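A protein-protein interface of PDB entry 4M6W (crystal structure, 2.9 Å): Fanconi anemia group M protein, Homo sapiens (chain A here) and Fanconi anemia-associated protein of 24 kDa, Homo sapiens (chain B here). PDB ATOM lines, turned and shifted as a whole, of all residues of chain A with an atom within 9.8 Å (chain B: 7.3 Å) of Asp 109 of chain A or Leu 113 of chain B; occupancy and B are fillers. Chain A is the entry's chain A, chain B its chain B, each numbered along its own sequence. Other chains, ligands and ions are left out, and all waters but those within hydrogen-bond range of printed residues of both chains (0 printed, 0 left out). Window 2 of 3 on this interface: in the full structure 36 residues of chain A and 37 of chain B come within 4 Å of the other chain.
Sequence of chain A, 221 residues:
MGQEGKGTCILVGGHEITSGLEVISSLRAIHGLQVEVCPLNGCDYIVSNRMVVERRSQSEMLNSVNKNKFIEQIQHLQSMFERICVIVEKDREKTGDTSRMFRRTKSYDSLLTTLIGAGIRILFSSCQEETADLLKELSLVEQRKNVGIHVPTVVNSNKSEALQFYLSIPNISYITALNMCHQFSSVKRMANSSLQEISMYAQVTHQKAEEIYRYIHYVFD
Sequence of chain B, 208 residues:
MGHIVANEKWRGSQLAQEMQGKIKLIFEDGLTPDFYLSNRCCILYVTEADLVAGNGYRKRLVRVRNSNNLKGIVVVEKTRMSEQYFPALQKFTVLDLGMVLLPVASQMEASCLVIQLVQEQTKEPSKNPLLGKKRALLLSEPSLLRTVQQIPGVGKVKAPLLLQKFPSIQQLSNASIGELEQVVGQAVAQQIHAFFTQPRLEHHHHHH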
ATOM      1  N   GLN A  58      23.653 -18.239  -8.535  1.00  0.00           N
ATOM      2  CA  GLN A  58      23.810 -16.940  -7.878  1.00  0.00           C
ATOM      3  C   GLN A  58      25.294 -16.592  -7.719  1.00  0.00           C
ATOM      4  O   GLN A  58      25.659 -15.422  -7.786  1.00  0.00           O
ATOM      5  CB  GLN A  58      23.090 -16.893  -6.522  1.00  0.00           C
ATOM      6  CG  GLN A  58      22.586 -15.496  -6.157  1.00  0.00           C
ATOM      7  CD  GLN A  58      21.939 -15.415  -4.778  1.00  0.00           C
ATOM      8  OE1 GLN A  58      21.449 -16.415  -4.238  1.00  0.00           O
ATOM      9  NE2 GLN A  58      21.926 -14.208  -4.203  1.00  0.00           N
ATOM     10  N   MET A  61      26.545 -15.292 -11.167  1.00  0.00           N
ATOM     11  CA  MET A  61      26.084 -13.915 -11.373  1.00  0.00           C
ATOM     12  C   MET A  61      26.827 -12.912 -10.489  1.00  0.00           C
ATOM     13  O   MET A  61      27.107 -11.800 -10.919  1.00  0.00           O
ATOM     14  CB  MET A  61      24.564 -13.809 -11.156  1.00  0.00           C
ATOM     15  CG  MET A  61      23.725 -14.626 -12.137  1.00  0.00           C
ATOM     16  SD  MET A  61      23.480 -13.891 -13.772  1.00  0.00           S
ATOM     17  CE  MET A  61      25.040 -14.224 -14.596  1.00  0.00           C
ATOM     18  N   LEU A  62      27.159 -13.310  -9.268  1.00  0.00           N
ATOM     19  CA  LEU A  62      27.901 -12.439  -8.354  1.00  0.00           C
ATOM     20  C   LEU A  62      29.391 -12.349  -8.728  1.00  0.00           C
ATOM     21  O   LEU A  62      30.022 -11.312  -8.518  1.00  0.00           O
ATOM     22  CB  LEU A  62      27.710 -12.891  -6.894  1.00  0.00           C
ATOM     23  CG  LEU A  62      26.403 -12.445  -6.216  1.00  0.00           C
ATOM     24  CD1 LEU A  62      26.050 -13.358  -5.056  1.00  0.00           C
ATOM     25  CD2 LEU A  62      26.480 -10.999  -5.739  1.00  0.00           C
ATOM     26  N   SER A  64      31.608 -11.239 -10.871  1.00  0.00           N
ATOM     27  CA  SER A  64      31.613 -10.312 -12.007  1.00  0.00           C
ATOM     28  C   SER A  64      32.936 -10.313 -12.792  1.00  0.00           C
ATOM     29  O   SER A  64      33.534  -9.259 -13.012  1.00  0.00           O
ATOM     30  CB  SER A  64      31.227  -8.896 -11.549  1.00  0.00           C
ATOM     31  OG  SER A  64      29.817  -8.800 -11.356  1.00  0.00           O
ATOM     32  N   LYS A  67      30.854 -11.300 -16.061  1.00  0.00           N
ATOM     33  CA  LYS A  67      29.937 -10.176 -16.260  1.00  0.00           C
ATOM     34  C   LYS A  67      29.797  -9.825 -17.740  1.00  0.00           C
ATOM     35  O   LYS A  67      28.684  -9.719 -18.255  1.00  0.00           O
ATOM     36  CB  LYS A  67      30.434  -8.963 -15.443  1.00  0.00           C
ATOM     37  CG  LYS A  67      30.013  -7.571 -15.918  1.00  0.00           C
ATOM     38  CD  LYS A  67      28.557  -7.252 -15.615  1.00  0.00           C
ATOM     39  CE  LYS A  67      28.227  -5.782 -15.871  1.00  0.00           C
ATOM     40  NZ  LYS A  67      28.553  -4.896 -14.715  1.00  0.00           N
ATOM     41  N   LYS A 106      25.499  -6.507  -4.504  1.00  0.00           N
ATOM     42  CA  LYS A 106      26.940  -6.415  -4.320  1.00  0.00           C
ATOM     43  C   LYS A 106      27.652  -6.153  -5.655  1.00  0.00           C
ATOM     44  O   LYS A 106      28.282  -7.049  -6.223  1.00  0.00           O
ATOM     45  CB  LYS A 106      27.473  -7.693  -3.655  1.00  0.00           C
ATOM     46  CG  LYS A 106      26.883  -7.971  -2.280  1.00  0.00           C
ATOM     47  CD  LYS A 106      27.541  -9.173  -1.612  1.00  0.00           C
ATOM     48  CE  LYS A 106      26.947  -9.448  -0.234  1.00  0.00           C
ATOM     49  NZ  LYS A 106      27.752 -10.426   0.553  1.00  0.00           N
ATOM     50  N   SER A 107      27.521  -4.919  -6.149  1.00  0.00           N
ATOM     51  CA  SER A 107      28.165  -4.448  -7.396  1.00  0.00           C
ATOM     52  C   SER A 107      27.588  -5.027  -8.705  1.00  0.00           C
ATOM     53  O   SER A 107      27.880  -4.513  -9.788  1.00  0.00           O
ATOM     54  CB  SER A 107      29.691  -4.659  -7.358  1.00  0.00           C
ATOM     55  OG  SER A 107      30.284  -4.015  -6.239  1.00  0.00           O
ATOM     56  N   TYR A 108      26.775  -6.081  -8.605  1.00  0.00           N
ATOM     57  CA  TYR A 108      26.176  -6.734  -9.776  1.00  0.00           C
ATOM     58  C   TYR A 108      24.737  -6.257 -10.016  1.00  0.00           C
ATOM     59  O   TYR A 108      24.074  -6.702 -10.956  1.00  0.00           O
ATOM     60  CB  TYR A 108      26.266  -8.266  -9.636  1.00  0.00           C
ATOM     61  CG  TYR A 108      25.020  -9.006  -9.152  1.00  0.00           C
ATOM     62  CD1 TYR A 108      24.508  -8.817  -7.868  1.00  0.00           C
ATOM     63  CD2 TYR A 108      24.385  -9.938  -9.973  1.00  0.00           C
ATOM     64  CE1 TYR A 108      23.384  -9.512  -7.433  1.00  0.00           C
ATOM     65  CE2 TYR A 108      23.268 -10.637  -9.544  1.00  0.00           C
ATOM     66  CZ  TYR A 108      22.773 -10.422  -8.277  1.00  0.00           C
ATOM     67  OH  TYR A 108      21.664 -11.119  -7.868  1.00  0.00           O
ATOM     68  N   ASP A 109      24.275  -5.333  -9.172  1.00  0.00           N
ATOM     69  CA  ASP A 109      22.981  -4.667  -9.362  1.00  0.00           C
ATOM     70  C   ASP A 109      22.937  -3.914 -10.693  1.00  0.00           C
ATOM     71  O   ASP A 109      21.860  -3.665 -11.229  1.00  0.00           O
ATOM     72  CB  ASP A 109      22.692  -3.689  -8.210  1.00  0.00           C
ATOM     73  CG  ASP A 109      22.571  -4.381  -6.854  1.00  0.00           C
ATOM     74  OD1 ASP A 109      23.057  -5.525  -6.711  1.00  0.00           O
ATOM     75  OD2 ASP A 109      21.998  -3.768  -5.926  1.00  0.00           O
ATOM     76  N   SER A 110      24.111  -3.538 -11.207  1.00  0.00           N
ATOM     77  CA  SER A 110      24.231  -2.927 -12.531  1.00  0.00           C
ATOM     78  C   SER A 110      23.919  -3.938 -13.640  1.00  0.00           C
ATOM     79  O   SER A 110      23.269  -3.597 -14.617  1.00  0.00           O
ATOM     80  CB  SER A 110      25.627  -2.320 -12.725  1.00  0.00           C
ATOM     81  OG  SER A 110      26.638  -3.287 -12.501  1.00  0.00           O
ATOM     82  N   LEU A 111      24.377  -5.180 -13.472  1.00  0.00           N
ATOM     83  CA  LEU A 111      24.064  -6.262 -14.413  1.00  0.00           C
ATOM     84  C   LEU A 111      22.550  -6.463 -14.496  1.00  0.00           C
ATOM     85  O   LEU A 111      21.986  -6.548 -15.590  1.00  0.00           O
ATOM     86  CB  LEU A 111      24.733  -7.576 -13.974  1.00  0.00           C
ATOM     87  CG  LEU A 111      25.022  -8.704 -14.983  1.00  0.00           C
ATOM     88  CD1 LEU A 111      24.965 -10.050 -14.272  1.00  0.00           C
ATOM     89  CD2 LEU A 111      24.101  -8.728 -16.196  1.00  0.00           C
ATOM     90  N   LEU A 112      21.900  -6.533 -13.336  1.00  0.00           N
ATOM     91  CA  LEU A 112      20.450  -6.731 -13.273  1.00  0.00           C
ATOM     92  C   LEU A 112      19.678  -5.598 -13.943  1.00  0.00           C
ATOM     93  O   LEU A 112      18.706  -5.849 -14.645  1.00  0.00           O
ATOM     94  CB  LEU A 112      19.974  -6.879 -11.823  1.00  0.00           C
ATOM     95  CG  LEU A 112      20.381  -8.121 -11.025  1.00  0.00           C
ATOM     96  CD1 LEU A 112      19.712  -8.087  -9.658  1.00  0.00           C
ATOM     97  CD2 LEU A 112      20.041  -9.420 -11.745  1.00  0.00           C
ATOM     98  N   THR A 113      20.110  -4.359 -13.725  1.00  0.00           N
ATOM     99  CA  THR A 113      19.415  -3.201 -14.283  1.00  0.00           C
ATOM    100  C   THR A 113      19.532  -3.113 -15.809  1.00  0.00           C
ATOM    101  O   THR A 113      18.580  -2.694 -16.471  1.00  0.00           O
ATOM    102  CB  THR A 113      19.899  -1.880 -13.655  1.00  0.00           C
ATOM    103  OG1 THR A 113      21.324  -1.812 -13.718  1.00  0.00           O
ATOM    104  CG2 THR A 113      19.451  -1.777 -12.205  1.00  0.00           C
ATOM    105  N   THR A 114      20.675  -3.508 -16.372  1.00  0.00           N
ATOM    106  CA  THR A 114      20.806  -3.521 -17.841  1.00  0.00           C
ATOM    107  C   THR A 114      19.867  -4.585 -18.414  1.00  0.00           C
ATOM    108  O   THR A 114      19.243  -4.370 -19.447  1.00  0.00           O
ATOM    109  CB  THR A 114      22.253  -3.744 -18.391  1.00  0.00           C
ATOM    110  OG1 THR A 114      22.438  -5.111 -18.774  1.00  0.00           O
ATOM    111  CG2 THR A 114      23.340  -3.341 -17.405  1.00  0.00           C
ATOM    112  N   LEU A 115      19.766  -5.722 -17.728  1.00  0.00           N
ATOM    113  CA  LEU A 115      18.870  -6.798 -18.145  1.00  0.00           C
ATOM    114  C   LEU A 115      17.423  -6.313 -18.142  1.00  0.00           C
ATOM    115  O   LEU A 115      16.740  -6.399 -19.159  1.00  0.00           O
ATOM    116  CB  LEU A 115      19.018  -8.026 -17.236  1.00  0.00           C
ATOM    117  CG  LEU A 115      20.310  -8.849 -17.332  1.00  0.00           C
ATOM    118  CD1 LEU A 115      20.432  -9.776 -16.132  1.00  0.00           C
ATOM    119  CD2 LEU A 115      20.364  -9.654 -18.621  1.00  0.00           C
ATOM    120  N   ILE A 116      16.979  -5.794 -16.998  1.00  0.00           N
ATOM    121  CA  ILE A 116      15.639  -5.202 -16.848  1.00  0.00           C
ATOM    122  C   ILE A 116      15.391  -4.136 -17.911  1.00  0.00           C
ATOM    123  O   ILE A 116      14.369  -4.166 -18.592  1.00  0.00           O
ATOM    124  CB  ILE A 116      15.451  -4.548 -15.455  1.00  0.00           C
ATOM    125  CG1 ILE A 116      15.483  -5.608 -14.350  1.00  0.00           C
ATOM    126  CG2 ILE A 116      14.131  -3.790 -15.375  1.00  0.00           C
ATOM    127  CD1 ILE A 116      15.780  -5.048 -12.978  1.00  0.00           C
ATOM    128  N   GLY A 117      16.337  -3.203 -18.038  1.00  0.00           N
ATOM    129  CA  GLY A 117      16.270  -2.135 -19.033  1.00  0.00           C
ATOM    130  C   GLY A 117      16.182  -2.623 -20.468  1.00  0.00           C
ATOM    131  O   GLY A 117      15.634  -1.940 -21.322  1.00  0.00           O
ATOM    132  N   ILE A 122      13.484 -11.764 -15.505  1.00  0.00           N
ATOM    133  CA  ILE A 122      14.386 -12.486 -14.596  1.00  0.00           C
ATOM    134  C   ILE A 122      13.609 -13.179 -13.454  1.00  0.00           C
ATOM    135  O   ILE A 122      12.791 -12.558 -12.781  1.00  0.00           O
ATOM    136  CB  ILE A 122      15.554 -11.573 -14.098  1.00  0.00           C
ATOM    137  CG1 ILE A 122      15.980 -11.894 -12.660  1.00  0.00           C
ATOM    138  CG2 ILE A 122      15.212 -10.091 -14.210  1.00  0.00           C
ATOM    139  CD1 ILE A 122      16.971 -13.028 -12.562  1.00  0.00           C
ATOM    140  N   PHE A 124      13.863 -16.033  -9.967  1.00  0.00           N
ATOM    141  CA  PHE A 124      14.743 -16.515  -8.896  1.00  0.00           C
ATOM    142  C   PHE A 124      14.273 -17.857  -8.338  1.00  0.00           C
ATOM    143  O   PHE A 124      13.102 -18.021  -7.997  1.00  0.00           O
ATOM    144  CB  PHE A 124      14.827 -15.479  -7.787  1.00  0.00           C
ATOM    145  CG  PHE A 124      15.468 -14.198  -8.222  1.00  0.00           C
ATOM    146  CD1 PHE A 124      14.706 -13.177  -8.752  1.00  0.00           C
ATOM    147  CD2 PHE A 124      16.841 -14.029  -8.126  1.00  0.00           C
ATOM    148  CE1 PHE A 124      15.295 -12.000  -9.168  1.00  0.00           C
ATOM    149  CE2 PHE A 124      17.438 -12.852  -8.536  1.00  0.00           C
ATOM    150  CZ  PHE A 124      16.661 -11.835  -9.060  1.00  0.00           C
ATOM    151  N   ILE B  43       8.122   2.092  -9.377  1.00  0.00           N
ATOM    152  CA  ILE B  43       8.496   1.023  -8.434  1.00  0.00           C
ATOM    153  C   ILE B  43       7.407   0.785  -7.385  1.00  0.00           C
ATOM    154  O   ILE B  43       6.899   1.732  -6.793  1.00  0.00           O
ATOM    155  CB  ILE B  43       9.827   1.344  -7.702  1.00  0.00           C
ATOM    156  CG1 ILE B  43      11.007   1.240  -8.673  1.00  0.00           C
ATOM    157  CG2 ILE B  43      10.049   0.405  -6.517  1.00  0.00           C
ATOM    158  CD1 ILE B  43      12.297   1.831  -8.146  1.00  0.00           C
ATOM    159  N   VAL B  74       8.367  -4.467  -9.371  1.00  0.00           N
ATOM    160  CA  VAL B  74       8.093  -4.722  -7.954  1.00  0.00           C
ATOM    161  C   VAL B  74       9.379  -5.085  -7.217  1.00  0.00           C
ATOM    162  O   VAL B  74      10.163  -5.882  -7.708  1.00  0.00           O
ATOM    163  CB  VAL B  74       7.042  -5.847  -7.790  1.00  0.00           C
ATOM    164  CG1 VAL B  74       6.667  -6.040  -6.329  1.00  0.00           C
ATOM    165  CG2 VAL B  74       5.793  -5.534  -8.603  1.00  0.00           C
ATOM    166  N   VAL B  75       9.599  -4.484  -6.047  1.00  0.00           N
ATOM    167  CA  VAL B  75      10.761  -4.795  -5.205  1.00  0.00           C
ATOM    168  C   VAL B  75      10.266  -5.337  -3.864  1.00  0.00           C
ATOM    169  O   VAL B  75       9.415  -4.723  -3.235  1.00  0.00           O
ATOM    170  CB  VAL B  75      11.639  -3.544  -4.968  1.00  0.00           C
ATOM    171  CG1 VAL B  75      12.866  -3.885  -4.129  1.00  0.00           C
ATOM    172  CG2 VAL B  75      12.074  -2.932  -6.293  1.00  0.00           C
ATOM    173  N   VAL B  76      10.807  -6.471  -3.419  1.00  0.00           N
ATOM    174  CA  VAL B  76      10.295  -7.154  -2.219  1.00  0.00           C
ATOM    175  C   VAL B  76      11.380  -7.488  -1.185  1.00  0.00           C
ATOM    176  O   VAL B  76      12.497  -7.858  -1.541  1.00  0.00           O
ATOM    177  CB  VAL B  76       9.530  -8.447  -2.593  1.00  0.00           C
ATOM    178  CG1 VAL B  76      10.404  -9.396  -3.405  1.00  0.00           C
ATOM    179  CG2 VAL B  76       8.993  -9.143  -1.345  1.00  0.00           C
ATOM    180  N   LEU B 102      12.063  -7.967  -7.761  1.00  0.00           N
ATOM    181  CA  LEU B 102      13.426  -7.855  -7.256  1.00  0.00           C
ATOM    182  C   LEU B 102      13.512  -8.176  -5.759  1.00  0.00           C
ATOM    183  O   LEU B 102      13.064  -7.389  -4.925  1.00  0.00           O
ATOM    184  CB  LEU B 102      13.967  -6.454  -7.543  1.00  0.00           C
ATOM    185  CG  LEU B 102      13.983  -6.065  -9.028  1.00  0.00           C
ATOM    186  CD1 LEU B 102      14.346  -4.596  -9.225  1.00  0.00           C
ATOM    187  CD2 LEU B 102      14.933  -6.947  -9.825  1.00  0.00           C
ATOM    188  N   PRO B 103      14.065  -9.350  -5.414  1.00  0.00           N
ATOM    189  CA  PRO B 103      14.322  -9.670  -4.011  1.00  0.00           C
ATOM    190  C   PRO B 103      15.384  -8.762  -3.399  1.00  0.00           C
ATOM    191  O   PRO B 103      16.304  -8.328  -4.084  1.00  0.00           O
ATOM    192  CB  PRO B 103      14.816 -11.122  -4.055  1.00  0.00           C
ATOM    193  CG  PRO B 103      15.233 -11.354  -5.466  1.00  0.00           C
ATOM    194  CD  PRO B 103      14.318 -10.504  -6.288  1.00  0.00           C
ATOM    195  N   VAL B 104      15.241  -8.493  -2.109  1.00  0.00           N
ATOM    196  CA  VAL B 104      16.073  -7.535  -1.400  1.00  0.00           C
ATOM    197  C   VAL B 104      16.071  -7.942   0.073  1.00  0.00           C
ATOM    198  O   VAL B 104      15.023  -8.288   0.607  1.00  0.00           O
ATOM    199  CB  VAL B 104      15.542  -6.095  -1.645  1.00  0.00           C
ATOM    200  CG1 VAL B 104      15.333  -5.321  -0.357  1.00  0.00           C
ATOM    201  CG2 VAL B 104      16.464  -5.334  -2.592  1.00  0.00           C
ATOM    202  N   MET B 108      17.993  -1.186   3.242  1.00  0.00           N
ATOM    203  CA  MET B 108      19.294  -0.580   2.965  1.00  0.00           C
ATOM    204  C   MET B 108      19.859  -1.108   1.636  1.00  0.00           C
ATOM    205  O   MET B 108      20.565  -0.387   0.932  1.00  0.00           O
ATOM    206  CB  MET B 108      20.264  -0.855   4.128  1.00  0.00           C
ATOM    207  CG  MET B 108      21.083   0.356   4.561  1.00  0.00           C
ATOM    208  SD  MET B 108      21.719   0.224   6.246  1.00  0.00           S
ATOM    209  CE  MET B 108      23.157  -0.820   5.992  1.00  0.00           C
ATOM    210  N   GLU B 109      19.546  -2.362   1.303  1.00  0.00           N
ATOM    211  CA  GLU B 109      19.865  -2.942  -0.016  1.00  0.00           C
ATOM    212  C   GLU B 109      19.027  -2.328  -1.140  1.00  0.00           C
ATOM    213  O   GLU B 109      19.512  -2.147  -2.260  1.00  0.00           O
ATOM    214  CB  GLU B 109      19.630  -4.458  -0.023  1.00  0.00           C
ATOM    215  CG  GLU B 109      20.871  -5.303   0.224  1.00  0.00           C
ATOM    216  CD  GLU B 109      20.666  -6.769  -0.131  1.00  0.00           C
ATOM    217  OE1 GLU B 109      19.559  -7.134  -0.591  1.00  0.00           O
ATOM    218  OE2 GLU B 109      21.616  -7.560   0.054  1.00  0.00           O
ATOM    219  N   ALA B 110      17.761  -2.042  -0.841  1.00  0.00           N
ATOM    220  CA  ALA B 110      16.854  -1.414  -1.797  1.00  0.00           C
ATOM    221  C   ALA B 110      17.309  -0.003  -2.158  1.00  0.00           C
ATOM    222  O   ALA B 110      17.056   0.468  -3.262  1.00  0.00           O
ATOM    223  CB  ALA B 110      15.441  -1.380  -1.243  1.00  0.00           C
ATOM    224  N   SER B 111      17.974   0.670  -1.225  1.00  0.00           N
ATOM    225  CA  SER B 111      18.556   1.977  -1.497  1.00  0.00           C
ATOM    226  C   SER B 111      19.516   1.893  -2.682  1.00  0.00           C
ATOM    227  O   SER B 111      19.310   2.550  -3.701  1.00  0.00           O
ATOM    228  CB  SER B 111      19.289   2.509  -0.261  1.00  0.00           C
ATOM    229  OG  SER B 111      18.408   2.637   0.842  1.00  0.00           O
ATOM    230  N   CYS B 112      20.548   1.064  -2.545  1.00  0.00           N
ATOM    231  CA  CYS B 112      21.545   0.877  -3.603  1.00  0.00           C
ATOM    232  C   CYS B 112      20.909   0.435  -4.923  1.00  0.00           C
ATOM    233  O   CYS B 112      21.323   0.875  -5.998  1.00  0.00           O
ATOM    234  CB  CYS B 112      22.609  -0.143  -3.171  1.00  0.00           C
ATOM    235  SG  CYS B 112      23.758   0.452  -1.903  1.00  0.00           S
ATOM    236  N   LEU B 113      19.899  -0.427  -4.832  1.00  0.00           N
ATOM    237  CA  LEU B 113      19.204  -0.933  -6.009  1.00  0.00           C
ATOM    238  C   LEU B 113      18.456   0.175  -6.740  1.00  0.00           C
ATOM    239  O   LEU B 113      18.625   0.342  -7.942  1.00  0.00           O
ATOM    240  CB  LEU B 113      18.234  -2.050  -5.615  1.00  0.00           C
ATOM    241  CG  LEU B 113      17.479  -2.781  -6.733  1.00  0.00           C
ATOM    242  CD1 LEU B 113      18.426  -3.516  -7.667  1.00  0.00           C
ATOM    243  CD2 LEU B 113      16.478  -3.750  -6.124  1.00  0.00           C
ATOM    244  N   VAL B 114      17.642   0.934  -6.013  1.00  0.00           N
ATOM    245  CA  VAL B 114      16.871   2.030  -6.606  1.00  0.00           C
ATOM    246  C   VAL B 114      17.797   3.096  -7.187  1.00  0.00           C
ATOM    247  O   VAL B 114      17.504   3.650  -8.245  1.00  0.00           O
ATOM    248  CB  VAL B 114      15.882   2.658  -5.595  1.00  0.00           C
ATOM    249  CG1 VAL B 114      15.225   3.912  -6.160  1.00  0.00           C
ATOM    250  CG2 VAL B 114      14.810   1.644  -5.215  1.00  0.00           C
ATOM    251  N   ILE B 115      18.915   3.370  -6.514  1.00  0.00           N
ATOM    252  CA  ILE B 115      19.911   4.301  -7.051  1.00  0.00           C
ATOM    253  C   ILE B 115      20.360   3.848  -8.439  1.00  0.00           C
ATOM    254  O   ILE B 115      20.219   4.592  -9.403  1.00  0.00           O
ATOM    255  CB  ILE B 115      21.134   4.486  -6.116  1.00  0.00           C
ATOM    256  CG1 ILE B 115      20.728   5.259  -4.856  1.00  0.00           C
ATOM    257  CG2 ILE B 115      22.253   5.249  -6.818  1.00  0.00           C
ATOM    258  CD1 ILE B 115      21.755   5.227  -3.739  1.00  0.00           C
ATOM    259  N   GLN B 116      20.868   2.623  -8.538  1.00  0.00           N
ATOM    260  CA  GLN B 116      21.368   2.092  -9.813  1.00  0.00           C
ATOM    261  C   GLN B 116      20.245   1.911 -10.849  1.00  0.00           C
ATOM    262  O   GLN B 116      20.497   1.920 -12.054  1.00  0.00           O
ATOM    263  CB  GLN B 116      22.124   0.771  -9.580  1.00  0.00           C
ATOM    264  CG  GLN B 116      23.020   0.317 -10.730  1.00  0.00           C
ATOM    265  CD  GLN B 116      23.958   1.404 -11.237  1.00  0.00           C
ATOM    266  OE1 GLN B 116      23.839   1.858 -12.378  1.00  0.00           O
ATOM    267  NE2 GLN B 116      24.890   1.835 -10.389  1.00  0.00           N
ATOM    268  N   LEU B 117      19.015   1.754 -10.361  1.00  0.00           N
ATOM    269  CA  LEU B 117      17.824   1.638 -11.206  1.00  0.00           C
ATOM    270  C   LEU B 117      17.497   2.986 -11.850  1.00  0.00           C
ATOM    271  O   LEU B 117      17.094   3.045 -13.014  1.00  0.00           O
ATOM    272  CB  LEU B 117      16.644   1.146 -10.360  1.00  0.00           C
ATOM    273  CG  LEU B 117      15.455   0.378 -10.956  1.00  0.00           C
ATOM    274  CD1 LEU B 117      15.797  -0.462 -12.179  1.00  0.00           C
ATOM    275  CD2 LEU B 117      14.856  -0.504  -9.865  1.00  0.00           C
ATOM    276  N   VAL B 118      17.677   4.063 -11.081  1.00  0.00           N
ATOM    277  CA  VAL B 118      17.539   5.432 -11.589  1.00  0.00           C
ATOM    278  C   VAL B 118      18.669   5.762 -12.561  1.00  0.00           C
ATOM    279  O   VAL B 118      18.410   6.285 -13.643  1.00  0.00           O
ATOM    280  CB  VAL B 118      17.508   6.473 -10.443  1.00  0.00           C
ATOM    281  CG1 VAL B 118      17.657   7.896 -10.973  1.00  0.00           C
ATOM    282  CG2 VAL B 118      16.216   6.353  -9.652  1.00  0.00           C
ATOM    283  N   GLN B 119      19.911   5.460 -12.172  1.00  0.00           N
ATOM    284  CA  GLN B 119      21.082   5.669 -13.043  1.00  0.00           C
ATOM    285  C   GLN B 119      20.878   5.030 -14.420  1.00  0.00           C
ATOM    286  O   GLN B 119      21.172   5.645 -15.444  1.00  0.00           O
ATOM    287  CB  GLN B 119      22.364   5.106 -12.406  1.00  0.00           C
ATOM    288  CG  GLN B 119      22.781   5.741 -11.080  1.00  0.00           C
ATOM    289  CD  GLN B 119      22.947   7.251 -11.163  1.00  0.00           C
ATOM    290  OE1 GLN B 119      23.761   7.753 -11.943  1.00  0.00           O
ATOM    291  NE2 GLN B 119      22.177   7.986 -10.355  1.00  0.00           N
ATOM    292  N   GLU B 120      20.366   3.799 -14.428  1.00  0.00           N
ATOM    293  CA  GLU B 120      20.027   3.085 -15.663  1.00  0.00           C
ATOM    294  C   GLU B 120      18.978   3.842 -16.480  1.00  0.00           C
ATOM    295  O   GLU B 120      19.113   3.978 -17.696  1.00  0.00           O
ATOM    296  CB  GLU B 120      19.518   1.672 -15.329  1.00  0.00           C
ATOM    297  CG  GLU B 120      19.026   0.844 -16.515  1.00  0.00           C
ATOM    298  CD  GLU B 120      20.104   0.559 -17.549  1.00  0.00           C
ATOM    299  OE1 GLU B 120      21.303   0.545 -17.185  1.00  0.00           O
ATOM    300  OE2 GLU B 120      19.746   0.335 -18.729  1.00  0.00           O
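The backbone carbonyl oxygen (O) of Ser 107 of chain A is in hydrogen-bond range of the side-chain hydroxyl (OG) of Ser 110 of chain A (3.2 Å).
N of Lys 106 of chain A lies within hydrogen-bond range of OD1 of Asp 109 of chain A (3.4 Å).
The side-chain hydroxyl (OG1) of Thr 113 of chain A is in hydrogen-bond range of the backbone carbonyl oxygen (O) of Asp 109 of chain A.
OG1 of Thr 113 of chain A is in hydrogen-bond range of O of Ser 110 of chain A, 2.8 Å away.
The side-chain amino group (NZ) of Lys 67 of chain A sits at hydrogen-bond distance from the side-chain hydroxyl (OG) of Ser 110 of chain A, at 3.3 Å.
N of Leu 102 of chain B lies within hydrogen-bond range of O of Val 74 of chain B, at 2.8 Å.
Printed residues of chain B within 4 Å of Thr 113 of chain A: Gln 116, Leu 117 and Glu 120.
No residue of chain A comes within 4 Å of Ala 110 of chain B.
No residue of chain A comes within 4 Å of Cys 112 of chain B.
Printed residues of chain A within 4 Å of Leu 113 of chain B: Asp 109.
No residue of chain A comes within 4 Å of Val 114 of chain B.
Printed residues of chain A within 4 Å of Gln 116 of chain B: Ser 110 (3.9 Å) and Thr 113 (3.8 Å).
Of the printed residues of chain A, Glu 120 of chain B touches Thr 113 (3.6 Å).
The nearest printed residue of chain A that does not touch Leu 113 of chain B is Thr 113 of chain A (4.8 Å).
Among the printed residues, pairs that only touch across the chains: Phe 124 of chain A with Pro 103 of chain B (3.4 Å), Thr 113 of chain A with Glu 120 of chain B (3.6 Å), Ile 116 of chain A with Leu 102 of chain B (3.8 Å), Thr 113 of chain A with Gln 116 of chain B (3.8 Å), Thr 113 of chain A with Leu 117 of chain B (3.9 Å), Ser 110 of chain A with Gln 116 of chain B (3.9 Å) and Asp 109 of chain A with Leu 113 of chain B (3.98 Å).
Hydrophobic or aromatic side chains of chain A within 4 Å of the printed part of chain B: Ile 116 and Phe 124.
Printed residues of chain B that touch a printed residue of chain A: Leu 102, Pro 103, Leu 113, Gln 116, Leu 117 and Glu 120.
Hydrophobic or aromatic side chains of chain B that line the printed part of chain A: Leu 102, Pro 103, Leu 113 and Leu 117.
Among the printed residues, 7 pairs touch across the chains.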
